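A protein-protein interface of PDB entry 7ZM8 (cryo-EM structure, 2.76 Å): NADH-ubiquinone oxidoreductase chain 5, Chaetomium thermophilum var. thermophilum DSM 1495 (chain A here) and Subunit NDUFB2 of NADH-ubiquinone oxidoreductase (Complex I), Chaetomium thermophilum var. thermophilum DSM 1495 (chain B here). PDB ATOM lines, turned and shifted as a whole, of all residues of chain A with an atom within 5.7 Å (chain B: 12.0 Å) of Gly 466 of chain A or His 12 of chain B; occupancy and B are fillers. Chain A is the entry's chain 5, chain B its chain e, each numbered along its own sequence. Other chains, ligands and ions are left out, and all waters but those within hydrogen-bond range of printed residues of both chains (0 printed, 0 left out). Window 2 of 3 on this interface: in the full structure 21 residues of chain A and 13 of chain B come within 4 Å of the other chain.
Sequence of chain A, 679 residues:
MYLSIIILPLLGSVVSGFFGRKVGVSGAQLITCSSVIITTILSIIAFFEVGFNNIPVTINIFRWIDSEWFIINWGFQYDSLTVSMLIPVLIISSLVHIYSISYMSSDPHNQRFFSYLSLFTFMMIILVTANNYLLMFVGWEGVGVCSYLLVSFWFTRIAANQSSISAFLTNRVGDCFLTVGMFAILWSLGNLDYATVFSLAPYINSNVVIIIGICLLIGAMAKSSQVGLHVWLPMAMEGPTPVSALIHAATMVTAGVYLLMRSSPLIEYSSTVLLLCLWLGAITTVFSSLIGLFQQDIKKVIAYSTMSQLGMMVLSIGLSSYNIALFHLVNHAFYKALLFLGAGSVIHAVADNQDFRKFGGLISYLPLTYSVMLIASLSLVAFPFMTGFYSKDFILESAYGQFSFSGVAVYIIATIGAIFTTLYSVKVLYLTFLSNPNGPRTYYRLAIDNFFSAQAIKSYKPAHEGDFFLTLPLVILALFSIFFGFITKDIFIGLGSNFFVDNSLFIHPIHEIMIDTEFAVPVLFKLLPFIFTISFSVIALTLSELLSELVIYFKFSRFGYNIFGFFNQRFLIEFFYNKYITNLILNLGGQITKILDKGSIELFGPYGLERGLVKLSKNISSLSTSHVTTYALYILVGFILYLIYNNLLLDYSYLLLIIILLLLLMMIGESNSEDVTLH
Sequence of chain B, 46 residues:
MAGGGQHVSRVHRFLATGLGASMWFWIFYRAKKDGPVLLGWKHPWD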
ATOM      1  N   SER A 102     -23.910   3.679  -8.474  1.00  0.00           N
ATOM      2  CA  SER A 102     -23.786   2.528  -7.551  1.00  0.00           C
ATOM      3  C   SER A 102     -22.519   2.591  -6.698  1.00  0.00           C
ATOM      4  O   SER A 102     -22.607   2.234  -5.520  1.00  0.00           O
ATOM      5  CB  SER A 102     -23.804   1.265  -8.338  1.00  0.00           C
ATOM      6  OG  SER A 102     -23.593   0.146  -7.492  1.00  0.00           O
ATOM      7  N   PRO A 367     -19.214 -14.166 -10.779  1.00  0.00           N
ATOM      8  CA  PRO A 367     -19.063 -14.762 -12.099  1.00  0.00           C
ATOM      9  C   PRO A 367     -19.013 -13.735 -13.238  1.00  0.00           C
ATOM     10  O   PRO A 367     -18.186 -13.881 -14.109  1.00  0.00           O
ATOM     11  CB  PRO A 367     -20.325 -15.621 -12.227  1.00  0.00           C
ATOM     12  CG  PRO A 367     -21.321 -14.993 -11.285  1.00  0.00           C
ATOM     13  CD  PRO A 367     -20.474 -14.520 -10.126  1.00  0.00           C
ATOM     14  N   LEU A 368     -19.895 -12.734 -13.204  1.00  0.00           N
ATOM     15  CA  LEU A 368     -19.957 -11.725 -14.289  1.00  0.00           C
ATOM     16  C   LEU A 368     -18.654 -10.942 -14.299  1.00  0.00           C
ATOM     17  O   LEU A 368     -18.100 -10.750 -15.378  1.00  0.00           O
ATOM     18  CB  LEU A 368     -21.153 -10.803 -14.034  1.00  0.00           C
ATOM     19  CG  LEU A 368     -21.541  -9.863 -15.172  1.00  0.00           C
ATOM     20  CD1 LEU A 368     -21.354 -10.533 -16.521  1.00  0.00           C
ATOM     21  CD2 LEU A 368     -22.977  -9.407 -15.011  1.00  0.00           C
ATOM     22  N   HIS A 464     -20.792 -10.423  -2.744  1.00  0.00           N
ATOM     23  CA  HIS A 464     -21.811 -10.519  -3.822  1.00  0.00           C
ATOM     24  C   HIS A 464     -21.531  -9.513  -4.939  1.00  0.00           C
ATOM     25  O   HIS A 464     -20.801  -8.544  -4.686  1.00  0.00           O
ATOM     26  CB  HIS A 464     -23.209 -10.276  -3.241  1.00  0.00           C
ATOM     27  CG  HIS A 464     -23.368  -8.935  -2.607  1.00  0.00           C
ATOM     28  ND1 HIS A 464     -22.929  -8.669  -1.325  1.00  0.00           N
ATOM     29  CD2 HIS A 464     -23.914  -7.789  -3.065  1.00  0.00           C
ATOM     30  CE1 HIS A 464     -23.194  -7.414  -1.023  1.00  0.00           C
ATOM     31  NE2 HIS A 464     -23.798  -6.853  -2.075  1.00  0.00           N
ATOM     32  N   GLU A 465     -22.092  -9.742  -6.126  1.00  0.00           N
ATOM     33  CA  GLU A 465     -21.977  -8.776  -7.249  1.00  0.00           C
ATOM     34  C   GLU A 465     -22.876  -7.570  -6.963  1.00  0.00           C
ATOM     35  O   GLU A 465     -23.836  -7.730  -6.190  1.00  0.00           O
ATOM     36  CB  GLU A 465     -22.494  -9.416  -8.534  1.00  0.00           C
ATOM     37  CG  GLU A 465     -21.754 -10.674  -8.936  1.00  0.00           C
ATOM     38  CD  GLU A 465     -20.724 -10.445 -10.024  1.00  0.00           C
ATOM     39  OE1 GLU A 465     -20.637 -11.286 -10.927  1.00  0.00           O
ATOM     40  OE2 GLU A 465     -20.014  -9.426  -9.962  1.00  0.00           O
ATOM     41  N   GLY A 466     -22.609  -6.425  -7.593  1.00  0.00           N
ATOM     42  CA  GLY A 466     -23.386  -5.197  -7.336  1.00  0.00           C
ATOM     43  C   GLY A 466     -24.738  -5.133  -8.026  1.00  0.00           C
ATOM     44  O   GLY A 466     -25.259  -6.200  -8.401  1.00  0.00           O
ATOM     45  N   ASP A 467     -25.284  -3.926  -8.213  1.00  0.00           N
ATOM     46  CA  ASP A 467     -26.619  -3.758  -8.760  1.00  0.00           C
ATOM     47  C   ASP A 467     -26.569  -3.357 -10.233  1.00  0.00           C
ATOM     48  O   ASP A 467     -25.529  -3.418 -10.891  1.00  0.00           O
ATOM     49  CB  ASP A 467     -27.396  -2.741  -7.927  1.00  0.00           C
ATOM     50  CG  ASP A 467     -26.704  -1.396  -7.855  1.00  0.00           C
ATOM     51  OD1 ASP A 467     -26.776  -0.635  -8.841  1.00  0.00           O
ATOM     52  OD2 ASP A 467     -26.082  -1.105  -6.812  1.00  0.00           O
ATOM     53  N   PHE A 468     -27.724  -2.941 -10.755  1.00  0.00           N
ATOM     54  CA  PHE A 468     -27.878  -2.661 -12.179  1.00  0.00           C
ATOM     55  C   PHE A 468     -26.997  -1.500 -12.631  1.00  0.00           C
ATOM     56  O   PHE A 468     -26.349  -1.575 -13.681  1.00  0.00           O
ATOM     57  CB  PHE A 468     -29.356  -2.392 -12.462  1.00  0.00           C
ATOM     58  CG  PHE A 468     -29.616  -1.572 -13.689  1.00  0.00           C
ATOM     59  CD1 PHE A 468     -29.809  -2.185 -14.910  1.00  0.00           C
ATOM     60  CD2 PHE A 468     -29.713  -0.193 -13.611  1.00  0.00           C
ATOM     61  CE1 PHE A 468     -30.067  -1.437 -16.033  1.00  0.00           C
ATOM     62  CE2 PHE A 468     -29.964   0.558 -14.730  1.00  0.00           C
ATOM     63  CZ  PHE A 468     -30.143  -0.062 -15.945  1.00  0.00           C
ATOM     64  N   LEU A 470     -24.273  -0.795 -11.619  1.00  0.00           N
ATOM     65  CA  LEU A 470     -22.849  -1.205 -11.663  1.00  0.00           C
ATOM     66  C   LEU A 470     -22.613  -2.138 -12.851  1.00  0.00           C
ATOM     67  O   LEU A 470     -21.683  -1.871 -13.625  1.00  0.00           O
ATOM     68  CB  LEU A 470     -22.489  -1.889 -10.340  1.00  0.00           C
ATOM     69  CG  LEU A 470     -21.016  -1.810  -9.946  1.00  0.00           C
ATOM     70  CD1 LEU A 470     -20.680  -0.434  -9.396  1.00  0.00           C
ATOM     71  CD2 LEU A 470     -20.674  -2.883  -8.927  1.00  0.00           C
ATOM     72  N   THR A 471     -23.407  -3.197 -12.974  1.00  0.00           N
ATOM     73  CA  THR A 471     -23.202  -4.211 -14.043  1.00  0.00           C
ATOM     74  C   THR A 471     -23.446  -3.669 -15.457  1.00  0.00           C
ATOM     75  O   THR A 471     -22.724  -4.099 -16.362  1.00  0.00           O
ATOM     76  CB  THR A 471     -23.967  -5.493 -13.705  1.00  0.00           C
ATOM     77  OG1 THR A 471     -25.254  -5.113 -13.219  1.00  0.00           O
ATOM     78  CG2 THR A 471     -23.237  -6.301 -12.658  1.00  0.00           C
ATOM     79  N   VAL B   8     -25.649 -16.266  -5.386  1.00  0.00           N
ATOM     80  CA  VAL B   8     -25.372 -15.490  -6.618  1.00  0.00           C
ATOM     81  C   VAL B   8     -26.598 -15.486  -7.533  1.00  0.00           C
ATOM     82  O   VAL B   8     -27.153 -16.569  -7.765  1.00  0.00           O
ATOM     83  CB  VAL B   8     -24.164 -16.057  -7.388  1.00  0.00           C
ATOM     84  N   SER B   9     -26.988 -14.315  -8.047  1.00  0.00           N
ATOM     85  CA  SER B   9     -28.220 -14.185  -8.877  1.00  0.00           C
ATOM     86  C   SER B   9     -28.098 -14.860 -10.239  1.00  0.00           C
ATOM     87  O   SER B   9     -26.978 -14.921 -10.755  1.00  0.00           O
ATOM     88  CB  SER B   9     -28.623 -12.756  -9.058  1.00  0.00           C
ATOM     89  OG  SER B   9     -29.796 -12.670  -9.848  1.00  0.00           O
ATOM     90  N   ARG B  10     -29.224 -15.341 -10.777  1.00  0.00           N
ATOM     91  CA  ARG B  10     -29.266 -16.030 -12.090  1.00  0.00           C
ATOM     92  C   ARG B  10     -28.916 -15.088 -13.229  1.00  0.00           C
ATOM     93  O   ARG B  10     -28.377 -15.575 -14.212  1.00  0.00           O
ATOM     94  CB  ARG B  10     -30.687 -16.530 -12.341  1.00  0.00           C
ATOM     95  CG  ARG B  10     -31.264 -17.368 -11.212  1.00  0.00           C
ATOM     96  CD  ARG B  10     -32.776 -17.445 -11.300  1.00  0.00           C
ATOM     97  NE  ARG B  10     -33.237 -17.782 -12.639  1.00  0.00           N
ATOM     98  CZ  ARG B  10     -34.513 -17.895 -12.987  1.00  0.00           C
ATOM     99  NH1 ARG B  10     -34.836 -18.204 -14.231  1.00  0.00           N
ATOM    100  NH2 ARG B  10     -35.463 -17.697 -12.092  1.00  0.00           N
ATOM    101  N   VAL B  11     -29.340 -13.787 -13.052  1.00  0.00           N
ATOM    102  CA  VAL B  11     -29.141 -12.783 -14.133  1.00  0.00           C
ATOM    103  C   VAL B  11     -27.648 -12.608 -14.373  1.00  0.00           C
ATOM    104  O   VAL B  11     -27.238 -12.741 -15.527  1.00  0.00           O
ATOM    105  CB  VAL B  11     -29.819 -11.449 -13.771  1.00  0.00           C
ATOM    106  CG1 VAL B  11     -29.718 -10.436 -14.903  1.00  0.00           C
ATOM    107  CG2 VAL B  11     -31.270 -11.653 -13.365  1.00  0.00           C
ATOM    108  N   HIS B  12     -26.870 -12.338 -13.320  1.00  0.00           N
ATOM    109  CA  HIS B  12     -25.392 -12.215 -13.454  1.00  0.00           C
ATOM    110  C   HIS B  12     -24.802 -13.525 -13.980  1.00  0.00           C
ATOM    111  O   HIS B  12     -23.772 -13.460 -14.649  1.00  0.00           O
ATOM    112  CB  HIS B  12     -24.737 -11.801 -12.128  1.00  0.00           C
ATOM    113  CG  HIS B  12     -25.276 -10.533 -11.560  1.00  0.00           C
ATOM    114  ND1 HIS B  12     -26.030 -10.505 -10.403  1.00  0.00           N
ATOM    115  CD2 HIS B  12     -25.184  -9.256 -11.986  1.00  0.00           C
ATOM    116  CE1 HIS B  12     -26.373  -9.261 -10.136  1.00  0.00           C
ATOM    117  NE2 HIS B  12     -25.867  -8.475 -11.093  1.00  0.00           N
ATOM    118  N   ARG B  13     -25.437 -14.660 -13.682  1.00  0.00           N
ATOM    119  CA  ARG B  13     -24.966 -15.975 -14.173  1.00  0.00           C
ATOM    120  C   ARG B  13     -25.216 -16.095 -15.678  1.00  0.00           C
ATOM    121  O   ARG B  13     -24.309 -16.586 -16.377  1.00  0.00           O
ATOM    122  CB  ARG B  13     -25.609 -17.109 -13.372  1.00  0.00           C
ATOM    123  CG  ARG B  13     -24.850 -17.475 -12.104  1.00  0.00           C
ATOM    124  CD  ARG B  13     -25.793 -17.963 -11.025  1.00  0.00           C
ATOM    125  NE  ARG B  13     -26.811 -18.852 -11.562  1.00  0.00           N
ATOM    126  CZ  ARG B  13     -27.874 -19.266 -10.887  1.00  0.00           C
ATOM    127  NH1 ARG B  13     -28.748 -20.076 -11.460  1.00  0.00           N
ATOM    128  NH2 ARG B  13     -28.069 -18.860  -9.646  1.00  0.00           N
ATOM    129  N   PHE B  14     -26.382 -15.656 -16.160  1.00  0.00           N
ATOM    130  CA  PHE B  14     -26.716 -15.810 -17.587  1.00  0.00           C
ATOM    131  C   PHE B  14     -25.866 -14.818 -18.352  1.00  0.00           C
ATOM    132  O   PHE B  14     -25.372 -15.120 -19.429  1.00  0.00           O
ATOM    133  CB  PHE B  14     -28.196 -15.526 -17.802  1.00  0.00           C
ATOM    134  CG  PHE B  14     -28.588 -15.309 -19.242  1.00  0.00           C
ATOM    135  CD1 PHE B  14     -28.498 -16.337 -20.164  1.00  0.00           C
ATOM    136  CD2 PHE B  14     -29.042 -14.074 -19.676  1.00  0.00           C
ATOM    137  CE1 PHE B  14     -28.847 -16.136 -21.489  1.00  0.00           C
ATOM    138  CE2 PHE B  14     -29.394 -13.874 -20.999  1.00  0.00           C
ATOM    139  CZ  PHE B  14     -29.299 -14.906 -21.903  1.00  0.00           C
ATOM    140  N   LEU B  15     -25.741 -13.631 -17.789  1.00  0.00           N
ATOM    141  CA  LEU B  15     -24.905 -12.625 -18.430  1.00  0.00           C
ATOM    142  C   LEU B  15     -23.453 -13.071 -18.497  1.00  0.00           C
ATOM    143  O   LEU B  15     -22.779 -12.843 -19.506  1.00  0.00           O
ATOM    144  CB  LEU B  15     -25.016 -11.296 -17.690  1.00  0.00           C
ATOM    145  CG  LEU B  15     -26.105 -10.343 -18.171  1.00  0.00           C
ATOM    146  CD1 LEU B  15     -25.982  -9.018 -17.451  1.00  0.00           C
ATOM    147  CD2 LEU B  15     -26.023 -10.149 -19.671  1.00  0.00           C
ATOM    148  N   ALA B  16     -22.951 -13.693 -17.432  1.00  0.00           N
ATOM    149  CA  ALA B  16     -21.547 -14.088 -17.390  1.00  0.00           C
ATOM    150  C   ALA B  16     -21.229 -15.110 -18.471  1.00  0.00           C
ATOM    151  O   ALA B  16     -20.256 -14.959 -19.217  1.00  0.00           O
ATOM    152  CB  ALA B  16     -21.203 -14.645 -16.010  1.00  0.00           C
ATOM    153  N   THR B  17     -22.040 -16.164 -18.572  1.00  0.00           N
ATOM    154  CA  THR B  17     -21.793 -17.176 -19.589  1.00  0.00           C
ATOM    155  C   THR B  17     -22.200 -16.696 -20.975  1.00  0.00           C
ATOM    156  O   THR B  17     -21.634 -17.148 -21.974  1.00  0.00           O
ATOM    157  CB  THR B  17     -22.516 -18.475 -19.238  1.00  0.00           C
ATOM    158  OG1 THR B  17     -22.126 -19.501 -20.158  1.00  0.00           O
ATOM    159  CG2 THR B  17     -24.024 -18.297 -19.292  1.00  0.00           C
ATOM    160  N   GLY B  18     -23.182 -15.799 -21.058  1.00  0.00           N
ATOM    161  CA  GLY B  18     -23.541 -15.239 -22.347  1.00  0.00           C
ATOM    162  C   GLY B  18     -22.439 -14.374 -22.922  1.00  0.00           C
ATOM    163  O   GLY B  18     -22.139 -14.446 -24.116  1.00  0.00           O
ATOM    164  N   LEU B  19     -21.824 -13.543 -22.083  1.00  0.00           N
ATOM    165  CA  LEU B  19     -20.694 -12.741 -22.530  1.00  0.00           C
ATOM    166  C   LEU B  19     -19.515 -13.624 -22.898  1.00  0.00           C
ATOM    167  O   LEU B  19     -18.777 -13.323 -23.842  1.00  0.00           O
ATOM    168  CB  LEU B  19     -20.302 -11.740 -21.450  1.00  0.00           C
ATOM    169  CG  LEU B  19     -21.283 -10.578 -21.352  1.00  0.00           C
ATOM    170  CD1 LEU B  19     -21.075  -9.787 -20.078  1.00  0.00           C
ATOM    171  CD2 LEU B  19     -21.164  -9.699 -22.576  1.00  0.00           C
ATOM    172  N   GLY B  20     -19.311 -14.706 -22.149  1.00  0.00           N
ATOM    173  CA  GLY B  20     -18.286 -15.664 -22.517  1.00  0.00           C
ATOM    174  C   GLY B  20     -18.601 -16.381 -23.814  1.00  0.00           C
ATOM    175  O   GLY B  20     -17.727 -16.550 -24.667  1.00  0.00           O
ATOM    176  N   ALA B  21     -19.848 -16.817 -23.980  1.00  0.00           N
ATOM    177  CA  ALA B  21     -20.256 -17.433 -25.234  1.00  0.00           C
ATOM    178  C   ALA B  21     -20.317 -16.429 -26.377  1.00  0.00           C
ATOM    179  O   ALA B  21     -20.378 -16.838 -27.540  1.00  0.00           O
ATOM    180  CB  ALA B  21     -21.611 -18.120 -25.071  1.00  0.00           C
ATOM    181  N   SER B  22     -20.312 -15.129 -26.077  1.00  0.00           N
ATOM    182  CA  SER B  22     -20.120 -14.140 -27.131  1.00  0.00           C
ATOM    183  C   SER B  22     -18.764 -14.327 -27.793  1.00  0.00           C
ATOM    184  O   SER B  22     -18.669 -14.457 -29.016  1.00  0.00           O
ATOM    185  CB  SER B  22     -20.265 -12.731 -26.562  1.00  0.00           C
ATOM    186  OG  SER B  22     -21.619 -12.438 -26.267  1.00  0.00           O
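OE1 of Glu 465 of chain A lies within hydrogen-bond range of N of Leu 368 of chain A (2.8 Å).
The backbone carbonyl oxygen (O) of Asp 467 of chain A is in hydrogen-bond range of the side-chain hydroxyl (OG1) of Thr 471 of chain A, at 2.9 Å.
Among the printed residues, pairs that only touch across the chains: Gly 466 of chain A with His 12 of chain B, Thr 471 of chain A with His 12 of chain B, Leu 368 of chain A with Ala 16 of chain B, Leu 368 of chain A with Leu 19 of chain B, Pro 367 of chain A with Ala 16 of chain B, Leu 368 of chain A with His 12 of chain B and Leu 368 of chain A with Leu 15 of chain B.
Pro 367 of chain A touches one residue of chain B.
Of chain B, only His 12, Leu 15, Ala 16 and Leu 19 come within 4 Å of Leu 368 of chain A.
No residue of chain B comes within 4 Å of Glu 465 of chain A.
Of chain B, only His 12 comes within 4 Å of Gly 466 of chain A.
No residue of chain B comes within 4 Å of Asp 467 of chain A.
No residue of chain B comes within 4 Å of Leu 470 of chain A.
Of chain B, only His 12 comes within 4 Å of Thr 471 of chain A.
Of chain A, only Leu 368, Gly 466 and Thr 471 come within 4 Å of His 12 of chain B.
Printed residues of chain A within 4 Å of Leu 15 of chain B: Leu 368 (3.8 Å).
Printed residues of chain A within 4 Å of Ala 16 of chain B: Pro 367 and Leu 368.
Of the printed residues of chain A, Leu 19 of chain B touches Leu 368.
Of the 10 printed residues of chain A, 4 touch a printed residue of chain B.
Hydrophobic or aromatic side chains of chain A within 4 Å of the printed part of chain B: Leu 368.
Hydrophobic or aromatic side chains of chain B within 4 Å of the printed part of chain A: His 12, Leu 15, Ala 16 and Leu 19.
Among the printed residues, no Asp or Glu carboxylate lies within 4 Å of a Lys or Arg side-chain nitrogen of the other chain.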
